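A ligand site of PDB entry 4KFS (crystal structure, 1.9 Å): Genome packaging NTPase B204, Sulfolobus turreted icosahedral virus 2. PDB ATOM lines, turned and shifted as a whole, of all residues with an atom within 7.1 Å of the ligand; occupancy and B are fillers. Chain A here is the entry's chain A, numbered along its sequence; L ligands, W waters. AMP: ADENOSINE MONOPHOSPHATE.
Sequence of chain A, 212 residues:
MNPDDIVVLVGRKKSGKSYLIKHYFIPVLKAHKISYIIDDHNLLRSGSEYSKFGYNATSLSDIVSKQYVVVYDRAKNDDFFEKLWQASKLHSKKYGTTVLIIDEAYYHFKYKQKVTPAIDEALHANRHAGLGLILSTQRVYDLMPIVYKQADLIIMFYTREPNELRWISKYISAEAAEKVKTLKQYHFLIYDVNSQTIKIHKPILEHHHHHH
N of Gly 16 is in hydrogen-bond range of O1P of the ligand, 2.7 Å away. The backbone NH (N) of Tyr 19 sits at hydrogen-bond distance from an oxygen (O3P) of the ligand, at 2.8 Å. O of Ile 204 is in hydrogen-bond range of N6 of the ligand (2.8 Å). The backbone NH (N) of Ser 15 lies within hydrogen-bond range of an oxygen (O1P) of the ligand, 3.0 Å away. The backbone NH of Ser 18 is in hydrogen-bond range of an oxygen (O3P) of the ligand, at 3.1 Å. The backbone NH (N) of Lys 14 sits at hydrogen-bond distance from an oxygen (O1P) of the ligand, 3.1 Å away. An oxygen (O1P) of the ligand lies within hydrogen-bond range of the backbone NH (N) of Lys 17.
The side-chain hydroxyl (OH) of Tyr 19 sits at hydrogen-bond distance from the backbone carbonyl oxygen (O) of Leu 205, 3.4 Å away. The side-chain hydroxyl (OG) of Ser 15 is in hydrogen-bond range of the backbone NH (N) of Lys 17. O of Arg 12 lies within hydrogen-bond range of OG of Ser 15, 2.8 Å away. NZ of Lys 17 lies within hydrogen-bond range of O of Gly 11, at 3.0 Å. The side-chain amide nitrogen (NE2) of Gln 185 is in hydrogen-bond range of the side-chain hydroxyl (OH) of Tyr 186, 3.4 Å away.
Merely in contact with the ligand: Arg 12 (3.9 Å) and Tyr 186 (3.5 Å). Nine residues have an atom within 4 Å of the ligand: Arg 12, Lys 14, Ser 15, Gly 16, Lys 17, Ser 18, Tyr 19, Tyr 186 and Ile 204. The nearest printed residue that does not touch the ligand is Lys 13 (4.2 Å).
Water W1 lies within hydrogen-bond range of the backbone carbonyl oxygen of Gly 16 and a nitrogen (N1) of the ligand.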
ATOM      1  N   GLY A  11       9.990 -15.100 -23.256  1.00  0.00           N
ATOM      2  CA  GLY A  11       9.731 -16.522 -23.354  1.00  0.00           C
ATOM      3  C   GLY A  11       8.874 -16.998 -22.203  1.00  0.00           C
ATOM      4  O   GLY A  11       8.875 -16.392 -21.129  1.00  0.00           O
ATOM      5  N   ARG A  12       8.157 -18.089 -22.415  1.00  0.00           N
ATOM      6  CA  ARG A  12       7.263 -18.623 -21.391  1.00  0.00           C
ATOM      7  C   ARG A  12       8.007 -19.314 -20.249  1.00  0.00           C
ATOM      8  O   ARG A  12       9.232 -19.466 -20.260  1.00  0.00           O
ATOM      9  CB  ARG A  12       6.241 -19.567 -22.024  1.00  0.00           C
ATOM     10  CG  ARG A  12       5.271 -18.881 -22.989  1.00  0.00           C
ATOM     11  CD  ARG A  12       4.749 -19.876 -24.016  1.00  0.00           C
ATOM     12  NE  ARG A  12       3.403 -19.559 -24.507  1.00  0.00           N
ATOM     13  CZ  ARG A  12       3.138 -18.673 -25.470  1.00  0.00           C
ATOM     14  NH1 ARG A  12       4.131 -17.982 -26.025  1.00  0.00           N
ATOM     15  NH2 ARG A  12       1.892 -18.465 -25.859  1.00  0.00           N
ATOM     16  N   LYS A  13       7.244 -19.742 -19.242  1.00  0.00           N
ATOM     17  CA  LYS A  13       7.815 -20.472 -18.130  1.00  0.00           C
ATOM     18  C   LYS A  13       8.451 -21.749 -18.647  1.00  0.00           C
ATOM     19  O   LYS A  13       7.857 -22.457 -19.472  1.00  0.00           O
ATOM     20  CB  LYS A  13       6.728 -20.780 -17.088  1.00  0.00           C
ATOM     21  CG  LYS A  13       7.226 -20.821 -15.662  1.00  0.00           C
ATOM     22  CD  LYS A  13       6.082 -20.620 -14.688  1.00  0.00           C
ATOM     23  CE  LYS A  13       6.607 -20.254 -13.307  1.00  0.00           C
ATOM     24  NZ  LYS A  13       7.439 -19.012 -13.359  1.00  0.00           N
ATOM     25  N   LYS A  14       9.673 -22.010 -18.188  1.00  0.00           N
ATOM     26  CA  LYS A  14      10.460 -23.184 -18.582  1.00  0.00           C
ATOM     27  C   LYS A  14      11.012 -23.115 -20.007  1.00  0.00           C
ATOM     28  O   LYS A  14      11.607 -24.079 -20.478  1.00  0.00           O
ATOM     29  CB  LYS A  14       9.698 -24.497 -18.325  1.00  0.00           C
ATOM     30  N   SER A  15      10.855 -21.976 -20.669  1.00  0.00           N
ATOM     31  CA  SER A  15      11.374 -21.802 -22.017  1.00  0.00           C
ATOM     32  C   SER A  15      12.902 -21.732 -22.022  1.00  0.00           C
ATOM     33  O   SER A  15      13.527 -22.082 -23.015  1.00  0.00           O
ATOM     34  CB  SER A  15      10.836 -20.528 -22.667  1.00  0.00           C
ATOM     35  OG  SER A  15      11.401 -19.403 -22.017  1.00  0.00           O
ATOM     36  N   GLY A  16      13.488 -21.287 -20.921  1.00  0.00           N
ATOM     37  CA  GLY A  16      14.930 -21.203 -20.814  1.00  0.00           C
ATOM     38  C   GLY A  16      15.385 -19.777 -20.548  1.00  0.00           C
ATOM     39  O   GLY A  16      16.580 -19.464 -20.562  1.00  0.00           O
ATOM     40  N   LYS A  17      14.394 -18.924 -20.311  1.00  0.00           N
ATOM     41  CA  LYS A  17      14.632 -17.516 -20.039  1.00  0.00           C
ATOM     42  C   LYS A  17      15.487 -17.284 -18.801  1.00  0.00           C
ATOM     43  O   LYS A  17      16.556 -16.664 -18.869  1.00  0.00           O
ATOM     44  CB  LYS A  17      13.269 -16.838 -19.858  1.00  0.00           C
ATOM     45  CG  LYS A  17      13.289 -15.358 -19.943  1.00  0.00           C
ATOM     46  CD  LYS A  17      11.863 -14.857 -19.886  1.00  0.00           C
ATOM     47  CE  LYS A  17      11.127 -15.465 -18.706  1.00  0.00           C
ATOM     48  NZ  LYS A  17       9.750 -14.943 -18.600  1.00  0.00           N
ATOM     49  N   SER A  18      15.032 -17.789 -17.666  1.00  0.00           N
ATOM     50  CA  SER A  18      15.759 -17.663 -16.402  1.00  0.00           C
ATOM     51  C   SER A  18      17.106 -18.368 -16.453  1.00  0.00           C
ATOM     52  O   SER A  18      18.097 -17.887 -15.901  1.00  0.00           O
ATOM     53  CB  SER A  18      14.915 -18.230 -15.259  1.00  0.00           C
ATOM     54  OG  SER A  18      13.621 -17.659 -15.262  1.00  0.00           O
ATOM     55  N   TYR A  19      17.140 -19.525 -17.108  1.00  0.00           N
ATOM     56  CA  TYR A  19      18.366 -20.304 -17.249  1.00  0.00           C
ATOM     57  C   TYR A  19      19.421 -19.486 -17.977  1.00  0.00           C
ATOM     58  O   TYR A  19      20.592 -19.512 -17.618  1.00  0.00           O
ATOM     59  CB  TYR A  19      18.085 -21.609 -17.997  1.00  0.00           C
ATOM     60  CG  TYR A  19      19.212 -22.620 -17.937  1.00  0.00           C
ATOM     61  CD1 TYR A  19      19.272 -23.562 -16.910  1.00  0.00           C
ATOM     62  CD2 TYR A  19      20.222 -22.635 -18.903  1.00  0.00           C
ATOM     63  CE1 TYR A  19      20.307 -24.480 -16.837  1.00  0.00           C
ATOM     64  CE2 TYR A  19      21.251 -23.552 -18.849  1.00  0.00           C
ATOM     65  CZ  TYR A  19      21.298 -24.479 -17.808  1.00  0.00           C
ATOM     66  OH  TYR A  19      22.315 -25.400 -17.760  1.00  0.00           O
ATOM     67  N   LEU A  20      19.006 -18.735 -18.991  1.00  0.00           N
ATOM     68  CA  LEU A  20      19.918 -17.900 -19.757  1.00  0.00           C
ATOM     69  C   LEU A  20      20.486 -16.755 -18.885  1.00  0.00           C
ATOM     70  O   LEU A  20      21.651 -16.407 -18.984  1.00  0.00           O
ATOM     71  CB  LEU A  20      19.196 -17.349 -20.985  1.00  0.00           C
ATOM     72  CG  LEU A  20      19.980 -16.438 -21.916  1.00  0.00           C
ATOM     73  CD1 LEU A  20      21.162 -17.195 -22.505  1.00  0.00           C
ATOM     74  CD2 LEU A  20      19.069 -15.913 -23.022  1.00  0.00           C
ATOM     75  N   ILE A  21      19.634 -16.173 -18.053  1.00  0.00           N
ATOM     76  CA  ILE A  21      20.068 -15.130 -17.132  1.00  0.00           C
ATOM     77  C   ILE A  21      21.037 -15.677 -16.088  1.00  0.00           C
ATOM     78  O   ILE A  21      22.032 -15.050 -15.763  1.00  0.00           O
ATOM     79  CB  ILE A  21      18.875 -14.509 -16.398  1.00  0.00           C
ATOM     80  CG1 ILE A  21      17.816 -14.036 -17.395  1.00  0.00           C
ATOM     81  CG2 ILE A  21      19.343 -13.360 -15.516  1.00  0.00           C
ATOM     82  CD1 ILE A  21      16.536 -13.546 -16.723  1.00  0.00           C
ATOM     83  N   LYS A  22      20.744 -16.866 -15.567  1.00  0.00           N
ATOM     84  CA  LYS A  22      21.528 -17.447 -14.475  1.00  0.00           C
ATOM     85  C   LYS A  22      22.846 -18.082 -14.892  1.00  0.00           C
ATOM     86  O   LYS A  22      23.780 -18.139 -14.091  1.00  0.00           O
ATOM     87  CB  LYS A  22      20.698 -18.468 -13.701  1.00  0.00           C
ATOM     88  CG  LYS A  22      19.566 -17.858 -12.893  1.00  0.00           C
ATOM     89  CD  LYS A  22      18.596 -18.932 -12.392  1.00  0.00           C
ATOM     90  CE  LYS A  22      17.333 -18.303 -11.804  1.00  0.00           C
ATOM     91  NZ  LYS A  22      16.215 -19.271 -11.639  1.00  0.00           N
ATOM     92  N   HIS A  23      22.923 -18.581 -16.114  1.00  0.00           N
ATOM     93  CA  HIS A  23      24.080 -19.369 -16.496  1.00  0.00           C
ATOM     94  C   HIS A  23      24.823 -18.771 -17.668  1.00  0.00           C
ATOM     95  O   HIS A  23      25.868 -19.271 -18.086  1.00  0.00           O
ATOM     96  CB  HIS A  23      23.690 -20.823 -16.774  1.00  0.00           C
ATOM     97  CG  HIS A  23      23.239 -21.568 -15.554  1.00  0.00           C
ATOM     98  ND1 HIS A  23      21.936 -21.999 -15.393  1.00  0.00           N
ATOM     99  CD2 HIS A  23      23.891 -21.923 -14.432  1.00  0.00           C
ATOM    100  CE1 HIS A  23      21.823 -22.618 -14.225  1.00  0.00           C
ATOM    101  NE2 HIS A  23      22.993 -22.576 -13.622  1.00  0.00           N
ATOM    102  N   GLU A  49      14.387 -16.063  -5.818  1.00  0.00           N
ATOM    103  CA  GLU A  49      14.891 -16.815  -6.955  1.00  0.00           C
ATOM    104  C   GLU A  49      16.361 -16.531  -7.217  1.00  0.00           C
ATOM    105  O   GLU A  49      17.139 -17.450  -7.472  1.00  0.00           O
ATOM    106  CB  GLU A  49      14.056 -16.496  -8.209  1.00  0.00           C
ATOM    107  CG  GLU A  49      14.515 -17.247  -9.458  1.00  0.00           C
ATOM    108  CD  GLU A  49      13.576 -17.055 -10.641  1.00  0.00           C
ATOM    109  OE1 GLU A  49      13.749 -17.758 -11.649  1.00  0.00           O
ATOM    110  OE2 GLU A  49      12.674 -16.186 -10.570  1.00  0.00           O
ATOM    111  N   GLN A 138       7.043 -12.904 -19.962  1.00  0.00           N
ATOM    112  CA  GLN A 138       6.463 -14.146 -20.455  1.00  0.00           C
ATOM    113  C   GLN A 138       5.987 -14.009 -21.895  1.00  0.00           C
ATOM    114  O   GLN A 138       6.318 -14.830 -22.737  1.00  0.00           O
ATOM    115  CB  GLN A 138       5.315 -14.573 -19.556  1.00  0.00           C
ATOM    116  CG  GLN A 138       5.729 -14.800 -18.111  1.00  0.00           C
ATOM    117  CD  GLN A 138       6.770 -15.894 -18.004  1.00  0.00           C
ATOM    118  OE1 GLN A 138       7.848 -15.708 -17.429  1.00  0.00           O
ATOM    119  NE2 GLN A 138       6.457 -17.045 -18.569  1.00  0.00           N
ATOM    120  N   PHE A 157      12.309 -16.745 -27.282  1.00  0.00           N
ATOM    121  CA  PHE A 157      12.193 -18.188 -27.385  1.00  0.00           C
ATOM    122  C   PHE A 157      10.973 -18.556 -28.237  1.00  0.00           C
ATOM    123  O   PHE A 157      10.240 -17.668 -28.692  1.00  0.00           O
ATOM    124  CB  PHE A 157      12.113 -18.791 -25.974  1.00  0.00           C
ATOM    125  CG  PHE A 157      13.402 -18.697 -25.208  1.00  0.00           C
ATOM    126  CD1 PHE A 157      14.278 -19.768 -25.163  1.00  0.00           C
ATOM    127  CD2 PHE A 157      13.756 -17.523 -24.551  1.00  0.00           C
ATOM    128  CE1 PHE A 157      15.480 -19.684 -24.475  1.00  0.00           C
ATOM    129  CE2 PHE A 157      14.955 -17.430 -23.860  1.00  0.00           C
ATOM    130  CZ  PHE A 157      15.819 -18.504 -23.823  1.00  0.00           C
ATOM    131  N   GLN A 185      13.547 -26.508 -28.733  1.00  0.00           N
ATOM    132  CA  GLN A 185      13.622 -26.312 -27.288  1.00  0.00           C
ATOM    133  C   GLN A 185      14.930 -25.673 -26.843  1.00  0.00           C
ATOM    134  O   GLN A 185      15.998 -26.144 -27.184  1.00  0.00           O
ATOM    135  CB  GLN A 185      13.379 -27.607 -26.525  1.00  0.00           C
ATOM    136  CG  GLN A 185      13.196 -27.376 -25.027  1.00  0.00           C
ATOM    137  CD  GLN A 185      12.837 -28.638 -24.267  1.00  0.00           C
ATOM    138  OE1 GLN A 185      13.268 -29.747 -24.628  1.00  0.00           O
ATOM    139  NE2 GLN A 185      12.035 -28.494 -23.215  1.00  0.00           N
ATOM    140  N   TYR A 186      14.812 -24.572 -26.100  1.00  0.00           N
ATOM    141  CA  TYR A 186      15.958 -23.840 -25.536  1.00  0.00           C
ATOM    142  C   TYR A 186      16.758 -23.060 -26.562  1.00  0.00           C
ATOM    143  O   TYR A 186      17.724 -22.387 -26.195  1.00  0.00           O
ATOM    144  CB  TYR A 186      16.894 -24.723 -24.705  1.00  0.00           C
ATOM    145  CG  TYR A 186      16.199 -25.553 -23.662  1.00  0.00           C
ATOM    146  CD1 TYR A 186      15.171 -25.027 -22.891  1.00  0.00           C
ATOM    147  CD2 TYR A 186      16.558 -26.878 -23.451  1.00  0.00           C
ATOM    148  CE1 TYR A 186      14.536 -25.788 -21.928  1.00  0.00           C
ATOM    149  CE2 TYR A 186      15.927 -27.658 -22.500  1.00  0.00           C
ATOM    150  CZ  TYR A 186      14.919 -27.111 -21.745  1.00  0.00           C
ATOM    151  OH  TYR A 186      14.278 -27.872 -20.801  1.00  0.00           O
ATOM    152  N   HIS A 187      16.386 -23.149 -27.833  1.00  0.00           N
ATOM    153  CA  HIS A 187      16.993 -22.263 -28.824  1.00  0.00           C
ATOM    154  C   HIS A 187      16.351 -20.873 -28.690  1.00  0.00           C
ATOM    155  O   HIS A 187      15.210 -20.756 -28.266  1.00  0.00           O
ATOM    156  CB  HIS A 187      16.782 -22.807 -30.239  1.00  0.00           C
ATOM    157  CG  HIS A 187      17.406 -24.145 -30.471  1.00  0.00           C
ATOM    158  ND1 HIS A 187      17.055 -25.269 -29.750  1.00  0.00           N
ATOM    159  CD2 HIS A 187      18.355 -24.542 -31.359  1.00  0.00           C
ATOM    160  CE1 HIS A 187      17.745 -26.300 -30.191  1.00  0.00           C
ATOM    161  NE2 HIS A 187      18.552 -25.893 -31.160  1.00  0.00           N
ATOM    162  N   PRO A 203      20.995 -23.653 -27.716  1.00  0.00           N
ATOM    163  CA  PRO A 203      20.862 -23.646 -26.254  1.00  0.00           C
ATOM    164  C   PRO A 203      22.213 -23.412 -25.608  1.00  0.00           C
ATOM    165  O   PRO A 203      23.207 -23.966 -26.085  1.00  0.00           O
ATOM    166  CB  PRO A 203      20.371 -25.067 -25.963  1.00  0.00           C
ATOM    167  CG  PRO A 203      19.604 -25.464 -27.182  1.00  0.00           C
ATOM    168  CD  PRO A 203      20.367 -24.841 -28.328  1.00  0.00           C
ATOM    169  N   ILE A 204      22.258 -22.612 -24.561  1.00  0.00           N
ATOM    170  CA  ILE A 204      23.510 -22.429 -23.831  1.00  0.00           C
ATOM    171  C   ILE A 204      23.937 -23.712 -23.115  1.00  0.00           C
ATOM    172  O   ILE A 204      23.100 -24.557 -22.784  1.00  0.00           O
ATOM    173  CB  ILE A 204      23.419 -21.276 -22.811  1.00  0.00           C
ATOM    174  CG1 ILE A 204      22.258 -21.491 -21.847  1.00  0.00           C
ATOM    175  CG2 ILE A 204      23.255 -19.939 -23.516  1.00  0.00           C
ATOM    176  CD1 ILE A 204      22.289 -20.529 -20.695  1.00  0.00           C
ATOM    177  N   LEU A 205      25.238 -23.874 -22.888  1.00  0.00           N
ATOM    178  CA  LEU A 205      25.719 -25.031 -22.152  1.00  0.00           C
ATOM    179  C   LEU A 205      25.723 -24.763 -20.650  1.00  0.00           C
ATOM    180  O   LEU A 205      24.927 -25.333 -19.912  1.00  0.00           O
ATOM    181  CB  LEU A 205      27.124 -25.431 -22.619  1.00  0.00           C
HETATM  182  P   AMP L   1      13.303 -21.417 -17.377  1.00  0.00           P
HETATM  183  O1P AMP L   1      12.505 -20.803 -18.505  1.00  0.00           O
HETATM  184  O2P AMP L   1      12.708 -21.411 -15.987  1.00  0.00           O
HETATM  185  O3P AMP L   1      14.694 -20.812 -17.338  1.00  0.00           O
HETATM  186  O5' AMP L   1      13.729 -22.903 -17.761  1.00  0.00           O
HETATM  187  C5' AMP L   1      15.066 -23.344 -17.588  1.00  0.00           C
HETATM  188  C4' AMP L   1      15.130 -24.813 -17.246  1.00  0.00           C
HETATM  189  O4' AMP L   1      15.445 -25.574 -18.428  1.00  0.00           O
HETATM  190  C3' AMP L   1      16.204 -25.215 -16.251  1.00  0.00           C
HETATM  191  O3' AMP L   1      15.850 -24.959 -14.907  1.00  0.00           O
HETATM  192  C2' AMP L   1      16.434 -26.698 -16.571  1.00  0.00           C
HETATM  193  O2' AMP L   1      15.469 -27.505 -15.903  1.00  0.00           O
HETATM  194  C1' AMP L   1      16.152 -26.746 -18.080  1.00  0.00           C
HETATM  195  N9  AMP L   1      17.395 -26.810 -18.871  1.00  0.00           N
HETATM  196  C8  AMP L   1      18.281 -27.836 -18.808  1.00  0.00           C
HETATM  197  N7  AMP L   1      19.325 -27.631 -19.650  1.00  0.00           N
HETATM  198  C5  AMP L   1      19.109 -26.456 -20.271  1.00  0.00           C
HETATM  199  C6  AMP L   1      19.854 -25.668 -21.279  1.00  0.00           C
HETATM  200  N6  AMP L   1      21.030 -26.115 -21.790  1.00  0.00           N
HETATM  201  N1  AMP L   1      19.313 -24.491 -21.668  1.00  0.00           N
HETATM  202  C2  AMP L   1      18.142 -24.067 -21.139  1.00  0.00           C
HETATM  203  N3  AMP L   1      17.414 -24.726 -20.226  1.00  0.00           N
HETATM  204  C4  AMP L   1      17.839 -25.916 -19.757  1.00  0.00           C
HETATM  205  O   HOH W   1      18.273 -21.257 -21.702  1.00  0.00           O
